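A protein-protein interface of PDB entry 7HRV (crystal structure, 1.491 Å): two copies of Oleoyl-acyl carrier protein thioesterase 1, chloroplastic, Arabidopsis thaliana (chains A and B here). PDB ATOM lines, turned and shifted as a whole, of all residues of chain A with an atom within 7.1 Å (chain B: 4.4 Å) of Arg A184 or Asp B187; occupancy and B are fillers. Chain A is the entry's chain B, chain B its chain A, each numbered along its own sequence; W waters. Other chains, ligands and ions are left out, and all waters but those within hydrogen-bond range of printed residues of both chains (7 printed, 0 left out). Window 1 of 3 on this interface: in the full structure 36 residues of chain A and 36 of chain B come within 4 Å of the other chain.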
ATOM      1  N   GLU A  31      16.806  12.166 -25.945  1.00  0.00           N
ATOM      2  CA  GLU A  31      15.640  11.269 -25.951  1.00  0.00           C
ATOM      3  C   GLU A  31      15.383  10.764 -27.384  1.00  0.00           C
ATOM      4  O   GLU A  31      15.038   9.596 -27.571  1.00  0.00           O
ATOM      5  CB  GLU A  31      14.394  11.995 -25.422  1.00  0.00           C
ATOM      6  CG  GLU A  31      14.530  12.225 -23.935  1.00  0.00           C
ATOM      7  CD  GLU A  31      13.291  12.874 -23.368  1.00  0.00           C
ATOM      8  OE1 GLU A  31      13.307  14.113 -23.207  1.00  0.00           O
ATOM      9  OE2 GLU A  31      12.312  12.143 -23.092  1.00  0.00           O
ATOM     10  N   LYS A 182       4.092  13.068 -14.401  1.00  0.00           N
ATOM     11  CA  LYS A 182       3.249  11.895 -14.592  1.00  0.00           C
ATOM     12  C   LYS A 182       3.159  11.518 -16.046  1.00  0.00           C
ATOM     13  O   LYS A 182       3.199  12.387 -16.910  1.00  0.00           O
ATOM     14  CB  LYS A 182       1.858  12.066 -13.965  1.00  0.00           C
ATOM     15  CG  LYS A 182       0.995  13.118 -14.565  1.00  0.00           C
ATOM     16  CD  LYS A 182      -0.221  13.365 -13.641  1.00  0.00           C
ATOM     17  CE  LYS A 182      -1.234  14.324 -14.198  1.00  0.00           C
ATOM     18  NZ  LYS A 182      -2.359  14.563 -13.233  1.00  0.00           N
ATOM     19  N   PRO A 183       3.124  10.215 -16.325  1.00  0.00           N
ATOM     20  CA  PRO A 183       3.088   9.789 -17.728  1.00  0.00           C
ATOM     21  C   PRO A 183       1.712  10.003 -18.353  1.00  0.00           C
ATOM     22  O   PRO A 183       0.682   9.902 -17.663  1.00  0.00           O
ATOM     23  CB  PRO A 183       3.380   8.275 -17.646  1.00  0.00           C
ATOM     24  CG  PRO A 183       2.825   7.879 -16.301  1.00  0.00           C
ATOM     25  CD  PRO A 183       3.134   9.054 -15.400  1.00  0.00           C
ATOM     26  N   ARG A 184       1.696  10.338 -19.641  1.00  0.00           N
ATOM     27  CA  ARG A 184       0.453  10.401 -20.415  1.00  0.00           C
ATOM     28  C   ARG A 184       0.512   9.198 -21.403  1.00  0.00           C
ATOM     29  O   ARG A 184       1.527   8.488 -21.441  1.00  0.00           O
ATOM     30  CB  ARG A 184       0.245  11.757 -21.148  1.00  0.00           C
ATOM     31  CG  ARG A 184       1.388  12.230 -22.022  1.00  0.00           C
ATOM     32  CD  ARG A 184       1.116  13.672 -22.439  1.00  0.00           C
ATOM     33  NE  ARG A 184       2.132  14.243 -23.331  1.00  0.00           N
ATOM     34  CZ  ARG A 184       2.055  14.198 -24.661  1.00  0.00           C
ATOM     35  NH1 ARG A 184       1.086  13.488 -25.258  1.00  0.00           N
ATOM     36  NH2 ARG A 184       2.972  14.804 -25.404  1.00  0.00           N
ATOM     37  N   ARG A 185      -0.560   8.945 -22.190  1.00  0.00           N
ATOM     38  CA  ARG A 185      -0.573   7.763 -23.062  1.00  0.00           C
ATOM     39  C   ARG A 185       0.591   7.718 -24.022  1.00  0.00           C
ATOM     40  O   ARG A 185       1.079   6.632 -24.311  1.00  0.00           O
ATOM     41  CB  ARG A 185      -1.910   7.601 -23.816  1.00  0.00           C
ATOM     42  CG  ARG A 185      -3.083   7.363 -22.890  1.00  0.00           C
ATOM     43  CD  ARG A 185      -4.228   6.616 -23.600  1.00  0.00           C
ATOM     44  NE  ARG A 185      -5.370   6.554 -22.704  1.00  0.00           N
ATOM     45  CZ  ARG A 185      -6.323   7.475 -22.639  1.00  0.00           C
ATOM     46  NH1 ARG A 185      -6.351   8.474 -23.512  1.00  0.00           N
ATOM     47  NH2 ARG A 185      -7.295   7.367 -21.741  1.00  0.00           N
ATOM     48  N   ALA A 186       1.062   8.881 -24.494  1.00  0.00           N
ATOM     49  CA  ALA A 186       2.202   8.891 -25.429  1.00  0.00           C
ATOM     50  C   ALA A 186       3.497   8.353 -24.795  1.00  0.00           C
ATOM     51  O   ALA A 186       4.424   7.989 -25.501  1.00  0.00           O
ATOM     52  CB  ALA A 186       2.417  10.284 -25.967  1.00  0.00           C
ATOM     53  N   ASP A 187       3.570   8.337 -23.447  1.00  0.00           N
ATOM     54  CA  ASP A 187       4.725   7.809 -22.714  1.00  0.00           C
ATOM     55  C   ASP A 187       4.677   6.295 -22.531  1.00  0.00           C
ATOM     56  O   ASP A 187       5.621   5.753 -21.970  1.00  0.00           O
ATOM     57  CB  ASP A 187       4.781   8.427 -21.327  1.00  0.00           C
ATOM     58  CG  ASP A 187       5.108   9.907 -21.387  1.00  0.00           C
ATOM     59  OD1 ASP A 187       6.159  10.258 -21.980  1.00  0.00           O
ATOM     60  OD2 ASP A 187       4.328  10.709 -20.838  1.00  0.00           O
ATOM     61  N   LEU A 188       3.578   5.633 -22.933  1.00  0.00           N
ATOM     62  CA  LEU A 188       3.452   4.188 -22.771  1.00  0.00           C
ATOM     63  C   LEU A 188       3.838   3.450 -24.048  1.00  0.00           C
ATOM     64  O   LEU A 188       3.648   3.960 -25.163  1.00  0.00           O
ATOM     65  CB  LEU A 188       2.019   3.789 -22.370  1.00  0.00           C
ATOM     66  CG  LEU A 188       1.428   4.561 -21.172  1.00  0.00           C
ATOM     67  CD1 LEU A 188      -0.015   4.148 -20.898  1.00  0.00           C
ATOM     68  CD2 LEU A 188       2.313   4.397 -19.899  1.00  0.00           C
ATOM     69  N   VAL A 194       5.431   2.091 -19.007  1.00  0.00           N
ATOM     70  CA  VAL A 194       6.101   3.362 -19.352  1.00  0.00           C
ATOM     71  C   VAL A 194       7.363   3.070 -20.160  1.00  0.00           C
ATOM     72  O   VAL A 194       8.169   2.198 -19.815  1.00  0.00           O
ATOM     73  CB  VAL A 194       6.421   4.157 -18.064  1.00  0.00           C
ATOM     74  CG1 VAL A 194       7.236   5.420 -18.370  1.00  0.00           C
ATOM     75  CG2 VAL A 194       5.128   4.513 -17.346  1.00  0.00           C
ATOM     76  N   THR A 198      11.134   7.655 -21.438  1.00  0.00           N
ATOM     77  CA  THR A 198      10.440   8.644 -20.588  1.00  0.00           C
ATOM     78  C   THR A 198      11.253   8.951 -19.317  1.00  0.00           C
ATOM     79  O   THR A 198      11.354  10.112 -18.908  1.00  0.00           O
ATOM     80  CB  THR A 198       9.014   8.128 -20.256  1.00  0.00           C
ATOM     81  OG1 THR A 198       8.301   8.007 -21.497  1.00  0.00           O
ATOM     82  CG2 THR A 198       8.241   9.106 -19.334  1.00  0.00           C
ATOM     83  N   TRP A 202      12.452  12.482 -17.725  1.00  0.00           N
ATOM     84  CA  TRP A 202      12.179  12.916 -16.348  1.00  0.00           C
ATOM     85  C   TRP A 202      13.434  13.245 -15.570  1.00  0.00           C
ATOM     86  O   TRP A 202      13.433  14.212 -14.796  1.00  0.00           O
ATOM     87  CB  TRP A 202      11.345  11.883 -15.590  1.00  0.00           C
ATOM     88  CG  TRP A 202       9.923  11.761 -16.045  1.00  0.00           C
ATOM     89  CD1 TRP A 202       9.173  12.693 -16.721  1.00  0.00           C
ATOM     90  CD2 TRP A 202       9.077  10.626 -15.848  1.00  0.00           C
ATOM     91  NE1 TRP A 202       7.878  12.225 -16.890  1.00  0.00           N
ATOM     92  CE2 TRP A 202       7.802  10.950 -16.380  1.00  0.00           C
ATOM     93  CE3 TRP A 202       9.287   9.343 -15.319  1.00  0.00           C
ATOM     94  CZ2 TRP A 202       6.740  10.046 -16.365  1.00  0.00           C
ATOM     95  CZ3 TRP A 202       8.247   8.423 -15.372  1.00  0.00           C
ATOM     96  CH2 TRP A 202       6.979   8.793 -15.844  1.00  0.00           C
ATOM     97  N   GLN A 230       1.289   3.423 -14.686  1.00  0.00           N
ATOM     98  CA  GLN A 230       0.517   4.460 -15.393  1.00  0.00           C
ATOM     99  C   GLN A 230      -0.149   5.488 -14.459  1.00  0.00           C
ATOM    100  O   GLN A 230      -0.354   6.641 -14.858  1.00  0.00           O
ATOM    101  CB  GLN A 230      -0.551   3.784 -16.279  1.00  0.00           C
ATOM    102  CG  GLN A 230      -1.070   4.693 -17.373  1.00  0.00           C
ATOM    103  CD  GLN A 230      -2.186   4.088 -18.197  1.00  0.00           C
ATOM    104  OE1 GLN A 230      -2.954   4.813 -18.843  1.00  0.00           O
ATOM    105  NE2 GLN A 230      -2.283   2.766 -18.229  1.00  0.00           N
ATOM    106  N   GLU B  31      -1.440  10.646 -32.222  1.00  0.00           N
ATOM    107  CA  GLU B  31      -0.337  11.606 -32.042  1.00  0.00           C
ATOM    108  C   GLU B  31       0.806  11.246 -32.998  1.00  0.00           C
ATOM    109  O   GLU B  31       1.418  12.142 -33.570  1.00  0.00           O
ATOM    110  CB  GLU B  31       0.165  11.599 -30.589  1.00  0.00           C
ATOM    111  CG  GLU B  31      -0.874  12.228 -29.683  1.00  0.00           C
ATOM    112  CD  GLU B  31      -0.369  12.294 -28.259  1.00  0.00           C
ATOM    113  OE1 GLU B  31      -0.732  11.391 -27.476  1.00  0.00           O
ATOM    114  OE2 GLU B  31       0.382  13.247 -27.936  1.00  0.00           O
ATOM    115  N   PRO B 183       3.979  20.552 -19.736  1.00  0.00           N
ATOM    116  CA  PRO B 183       4.923  20.102 -20.768  1.00  0.00           C
ATOM    117  C   PRO B 183       6.312  19.858 -20.203  1.00  0.00           C
ATOM    118  O   PRO B 183       6.739  20.569 -19.281  1.00  0.00           O
ATOM    119  CB  PRO B 183       4.959  21.296 -21.756  1.00  0.00           C
ATOM    120  CG  PRO B 183       4.696  22.489 -20.880  1.00  0.00           C
ATOM    121  CD  PRO B 183       3.682  22.006 -19.859  1.00  0.00           C
ATOM    122  N   ARG B 184       7.007  18.863 -20.747  1.00  0.00           N
ATOM    123  CA  ARG B 184       8.424  18.648 -20.426  1.00  0.00           C
ATOM    124  C   ARG B 184       9.222  19.041 -21.700  1.00  0.00           C
ATOM    125  O   ARG B 184       8.609  19.368 -22.724  1.00  0.00           O
ATOM    126  CB  ARG B 184       8.741  17.197 -19.950  1.00  0.00           C
ATOM    127  CG  ARG B 184       8.281  16.083 -20.865  1.00  0.00           C
ATOM    128  CD  ARG B 184       8.439  14.755 -20.131  1.00  0.00           C
ATOM    129  NE  ARG B 184       8.048  13.575 -20.917  1.00  0.00           N
ATOM    130  CZ  ARG B 184       8.893  12.879 -21.678  1.00  0.00           C
ATOM    131  NH1 ARG B 184      10.148  13.310 -21.863  1.00  0.00           N
ATOM    132  NH2 ARG B 184       8.482  11.776 -22.297  1.00  0.00           N
ATOM    133  N   ARG B 185      10.581  19.023 -21.662  1.00  0.00           N
ATOM    134  CA  ARG B 185      11.350  19.472 -22.826  1.00  0.00           C
ATOM    135  C   ARG B 185      11.024  18.720 -24.094  1.00  0.00           C
ATOM    136  O   ARG B 185      11.027  19.326 -25.159  1.00  0.00           O
ATOM    137  CB  ARG B 185      12.871  19.457 -22.557  1.00  0.00           C
ATOM    138  CG  ARG B 185      13.289  20.429 -21.476  1.00  0.00           C
ATOM    139  CD  ARG B 185      14.773  20.848 -21.626  1.00  0.00           C
ATOM    140  NE  ARG B 185      15.148  21.654 -20.471  1.00  0.00           N
ATOM    141  CZ  ARG B 185      15.632  21.153 -19.340  1.00  0.00           C
ATOM    142  NH1 ARG B 185      15.925  19.858 -19.249  1.00  0.00           N
ATOM    143  NH2 ARG B 185      15.872  21.949 -18.304  1.00  0.00           N
ATOM    144  N   ALA B 186      10.679  17.430 -23.988  1.00  0.00           N
ATOM    145  CA  ALA B 186      10.345  16.656 -25.197  1.00  0.00           C
ATOM    146  C   ALA B 186       9.074  17.163 -25.899  1.00  0.00           C
ATOM    147  O   ALA B 186       8.849  16.862 -27.068  1.00  0.00           O
ATOM    148  CB  ALA B 186      10.215  15.193 -24.854  1.00  0.00           C
ATOM    149  N   ASP B 187       8.222  17.919 -25.168  1.00  0.00           N
ATOM    150  CA  ASP B 187       7.005  18.507 -25.734  1.00  0.00           C
ATOM    151  C   ASP B 187       7.256  19.835 -26.448  1.00  0.00           C
ATOM    152  O   ASP B 187       6.308  20.397 -26.990  1.00  0.00           O
ATOM    153  CB  ASP B 187       6.009  18.790 -24.616  1.00  0.00           C
ATOM    154  CG  ASP B 187       5.479  17.505 -24.006  1.00  0.00           C
ATOM    155  OD1 ASP B 187       4.943  16.668 -24.768  1.00  0.00           O
ATOM    156  OD2 ASP B 187       5.606  17.336 -22.773  1.00  0.00           O
ATOM    157  N   LEU B 188       8.487  20.363 -26.401  1.00  0.00           N
ATOM    158  CA  LEU B 188       8.793  21.630 -27.059  1.00  0.00           C
ATOM    159  C   LEU B 188       9.399  21.415 -28.446  1.00  0.00           C
ATOM    160  O   LEU B 188      10.114  20.432 -28.693  1.00  0.00           O
ATOM    161  CB  LEU B 188       9.760  22.480 -26.207  1.00  0.00           C
ATOM    162  CG  LEU B 188       9.353  22.671 -24.731  1.00  0.00           C
ATOM    163  CD1 LEU B 188      10.402  23.461 -23.959  1.00  0.00           C
ATOM    164  CD2 LEU B 188       7.950  23.330 -24.610  1.00  0.00           C
ATOM    165  N   ASP B 189       9.171  22.391 -29.354  1.00  0.00           N
ATOM    166  CA  ASP B 189       9.784  22.348 -30.681  1.00  0.00           C
ATOM    167  C   ASP B 189      11.169  23.035 -30.600  1.00  0.00           C
ATOM    168  O   ASP B 189      11.598  23.504 -29.526  1.00  0.00           O
ATOM    169  CB  ASP B 189       8.830  22.963 -31.744  1.00  0.00           C
ATOM    170  CG  ASP B 189       8.505  24.438 -31.534  1.00  0.00           C
ATOM    171  OD1 ASP B 189       9.232  25.107 -30.761  1.00  0.00           O
ATOM    172  OD2 ASP B 189       7.508  24.925 -32.137  1.00  0.00           O
ATOM    173  N   HIS B 193       8.631  26.483 -28.178  1.00  0.00           N
ATOM    174  CA  HIS B 193       7.178  26.608 -28.061  1.00  0.00           C
ATOM    175  C   HIS B 193       6.633  25.177 -27.907  1.00  0.00           C
ATOM    176  O   HIS B 193       7.244  24.222 -28.408  1.00  0.00           O
ATOM    177  CB  HIS B 193       6.573  27.249 -29.320  1.00  0.00           C
ATOM    178  CG  HIS B 193       6.859  28.723 -29.402  1.00  0.00           C
ATOM    179  ND1 HIS B 193       5.864  29.655 -29.191  1.00  0.00           N
ATOM    180  CD2 HIS B 193       8.032  29.369 -29.615  1.00  0.00           C
ATOM    181  CE1 HIS B 193       6.455  30.846 -29.290  1.00  0.00           C
ATOM    182  NE2 HIS B 193       7.764  30.724 -29.539  1.00  0.00           N
ATOM    183  N   VAL B 194       5.483  25.022 -27.230  1.00  0.00           N
ATOM    184  CA  VAL B 194       4.889  23.679 -27.102  1.00  0.00           C
ATOM    185  C   VAL B 194       4.451  23.186 -28.495  1.00  0.00           C
ATOM    186  O   VAL B 194       3.799  23.911 -29.254  1.00  0.00           O
ATOM    187  CB  VAL B 194       3.712  23.716 -26.112  1.00  0.00           C
ATOM    188  CG1 VAL B 194       2.988  22.367 -26.055  1.00  0.00           C
ATOM    189  CG2 VAL B 194       4.221  24.109 -24.725  1.00  0.00           C
ATOM    190  N   ASN B 195       4.858  21.969 -28.839  1.00  0.00           N
ATOM    191  CA  ASN B 195       4.522  21.352 -30.122  1.00  0.00           C
ATOM    192  C   ASN B 195       2.994  21.195 -30.253  1.00  0.00           C
ATOM    193  O   ASN B 195       2.349  20.803 -29.284  1.00  0.00           O
ATOM    194  CB  ASN B 195       5.168  19.963 -30.167  1.00  0.00           C
ATOM    195  CG  ASN B 195       5.058  19.296 -31.519  1.00  0.00           C
ATOM    196  OD1 ASN B 195       3.964  18.957 -31.974  1.00  0.00           O
ATOM    197  ND2 ASN B 195       6.164  19.121 -32.207  1.00  0.00           N
ATOM    198  N   THR B 198       1.279  18.007 -28.843  1.00  0.00           N
ATOM    199  CA  THR B 198       1.117  17.846 -27.384  1.00  0.00           C
ATOM    200  C   THR B 198      -0.335  18.153 -26.951  1.00  0.00           C
ATOM    201  O   THR B 198      -0.895  17.443 -26.119  1.00  0.00           O
ATOM    202  CB  THR B 198       2.140  18.749 -26.651  1.00  0.00           C
ATOM    203  OG1 THR B 198       3.454  18.290 -27.028  1.00  0.00           O
ATOM    204  CG2 THR B 198       2.000  18.668 -25.119  1.00  0.00           C
ATOM    205  N   GLY B 201      -2.553  15.212 -27.450  1.00  0.00           N
ATOM    206  CA  GLY B 201      -2.345  14.264 -26.340  1.00  0.00           C
ATOM    207  C   GLY B 201      -3.074  14.685 -25.074  1.00  0.00           C
ATOM    208  O   GLY B 201      -3.747  13.880 -24.416  1.00  0.00           O
ATOM    209  N   TRP B 202      -2.957  15.983 -24.737  1.00  0.00           N
ATOM    210  CA  TRP B 202      -3.643  16.483 -23.534  1.00  0.00           C
ATOM    211  C   TRP B 202      -5.153  16.399 -23.641  1.00  0.00           C
ATOM    212  O   TRP B 202      -5.813  16.075 -22.646  1.00  0.00           O
ATOM    213  CB  TRP B 202      -3.222  17.910 -23.196  1.00  0.00           C
ATOM    214  CG  TRP B 202      -1.819  18.056 -22.686  1.00  0.00           C
ATOM    215  CD1 TRP B 202      -1.036  17.093 -22.100  1.00  0.00           C
ATOM    216  CD2 TRP B 202      -1.028  19.250 -22.726  1.00  0.00           C
ATOM    217  NE1 TRP B 202       0.175  17.633 -21.716  1.00  0.00           N
ATOM    218  CE2 TRP B 202       0.214  18.953 -22.109  1.00  0.00           C
ATOM    219  CE3 TRP B 202      -1.227  20.524 -23.271  1.00  0.00           C
ATOM    220  CZ2 TRP B 202       1.225  19.909 -21.974  1.00  0.00           C
ATOM    221  CZ3 TRP B 202      -0.188  21.448 -23.215  1.00  0.00           C
ATOM    222  CH2 TRP B 202       1.006  21.152 -22.536  1.00  0.00           C
ATOM    223  N   GLU B 205      -6.148  12.803 -22.907  1.00  0.00           N
ATOM    224  CA  GLU B 205      -5.925  12.314 -21.540  1.00  0.00           C
ATOM    225  C   GLU B 205      -7.208  12.203 -20.698  1.00  0.00           C
ATOM    226  O   GLU B 205      -7.243  11.408 -19.743  1.00  0.00           O
ATOM    227  CB  GLU B 205      -4.901  13.206 -20.800  1.00  0.00           C
ATOM    228  CG  GLU B 205      -3.450  12.832 -21.053  1.00  0.00           C
ATOM    229  CD  GLU B 205      -3.090  11.396 -20.687  1.00  0.00           C
ATOM    230  OE1 GLU B 205      -3.017  10.553 -21.606  1.00  0.00           O
ATOM    231  OE2 GLU B 205      -2.842  11.115 -19.491  1.00  0.00           O
HETATM  232  O   HOH W   1      -0.712  11.238 -24.842  1.00  0.00           O
HETATM  233  O   HOH W   2      -1.179  12.282 -17.590  1.00  0.00           O
HETATM  234  O   HOH W   3       2.828  14.137 -28.158  1.00  0.00           O
HETATM  235  O   HOH W   4       4.153  15.348 -21.801  1.00  0.00           O
HETATM  236  O   HOH W   5      11.765  15.724 -21.797  1.00  0.00           O
HETATM  237  O   HOH W   6       5.309  13.181 -20.593  1.00  0.00           O
HETATM  238  O   HOH W   7      10.360  10.815 -24.197  1.00  0.00           O
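Water W7 bridges OE2 of Glu A31 (2.6 Å) and NH2 of Arg B184 (2.8 Å). Water W3 bridges the side-chain carboxylate of Glu B31 (2.6 Å) and the guanidinium group of Arg A184 (2.8 Å). Water W1 lies within hydrogen-bond range of the side-chain carboxylate (OE1) of Glu B31 (2.6 Å), the guanidinium group (NH1) of Arg A184 (2.9 Å) and the backbone NH (N) of Ala A186 (3.0 Å). Water W5 lies within hydrogen-bond range of the side-chain carboxylate (OE1) of Glu A31 (2.6 Å), the guanidinium group (NH1) of Arg B184 (2.9 Å) and the backbone NH (N) of Ala B186 (3.0 Å). Water W4 lies within hydrogen-bond range of the side-chain carboxylate (OD2) of Asp B187 (2.6 Å) and the guanidinium group (NE) of Arg A184 (2.8 Å). Water W2 bridges OE2 of Glu B205 (2.8 Å) and O of Pro A183 (3.0 Å).
Printed residues of chain B that touch a printed residue of chain A: Glu B31, Arg B184, Ala B186, Asp B187, Thr B198, Gly B201 and Glu B205. Along chain B the printed residues that touch a printed residue of chain A span positions 31 to 205. Printed residues of chain A that touch a printed residue of chain B: Glu A31, Arg A184, Arg A185, Ala A186, Asp A187 and Thr A198. Hydrophobic or aromatic side chains of chain A within 4 Å of the printed part of chain B: Ala A186. Among the printed residues, Asp or Glu carboxylates within 4 Å of a Lys or Arg side-chain nitrogen of the other chain: Glu A31 with Arg B184, Arg A184 with Glu B31, Arg A184 with Asp B187 and Asp A187 with Arg B184.
Among the printed residues, merely in contact across the chains: Glu A31 with Ala B186 (3.7 Å), Arg A184 with Thr B198 (3.9 Å), Arg A184 with Gly B201 (3.7 Å), Arg A184 with Glu B205 (3.4 Å), Ala A186 with Glu B31 (3.7 Å) and Thr A198 with Arg B184 (3.9 Å).
Glu A31 touches Arg B184, and with the chains exchanged Arg A184 touches Glu B31. Glu A31 touches Ala B186, and with the chains exchanged Ala A186 touches Glu B31. Arg A184 touches Asp B187, and with the chains exchanged Asp A187 touches Arg B184. Arg A184 touches Thr B198, and with the chains exchanged Thr A198 touches Arg B184. 10 positions are printed for both chains. Of the 11 pairs that touch across the chains among the printed residues, 8 have their exchanged pair printed and touching as well.
N of Arg B184 sits at hydrogen-bond distance from OD2 of Asp B187 (2.9 Å). The side-chain carboxylate of Asp B187 sits at hydrogen-bond distance from the side-chain hydroxyl of Thr B198, 3.2 Å away. N of Asn B195 sits at hydrogen-bond distance from O of Asp B187 (2.8 Å). The backbone NH (N) of Arg A184 sits at hydrogen-bond distance from the side-chain carboxylate (OD2) of Asp A187 (2.9 Å). The side-chain carboxylate (OD1) of Asp A187 is in hydrogen-bond range of the side-chain hydroxyl (OG1) of Thr A198, at 3.1 Å.
The guanidinium group (NH1) of Arg B184 lies within salt-bridge range of the side-chain carboxylate (OE2) of Glu A31, at 2.7 Å. OE1 of Glu B205 lies within hydrogen-bond range of N of Arg A185 (3.0 Å). The side-chain carboxylate (OD1) of Asp B187 lies within salt-bridge range of the guanidinium group (NH2) of Arg A184 (2.8 Å). OD1 of Asp A187 is in salt-bridge range of NH2 of Arg B184 (2.8 Å). OE2 of Glu B31 lies within salt-bridge range of NH1 of Arg A184, 2.8 Å away.
Of chain B, only Glu B31, Asp B187, Thr B198, Gly B201 and Glu B205 come within 4 Å of Arg A184. Leu A188 touches none of the printed residues of chain B. Val A194 touches none of the printed residues of chain B. Printed residues of chain A within 4 Å of Ala B186: Glu A31. Of chain A, only Arg A184 comes within 4 Å of Asp B187. Of the printed residues of chain A, Thr B198 touches Arg A184 (3.9 Å). The nearest residue of chain B that does not touch Arg A184 is Trp B202 (4.1 Å).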
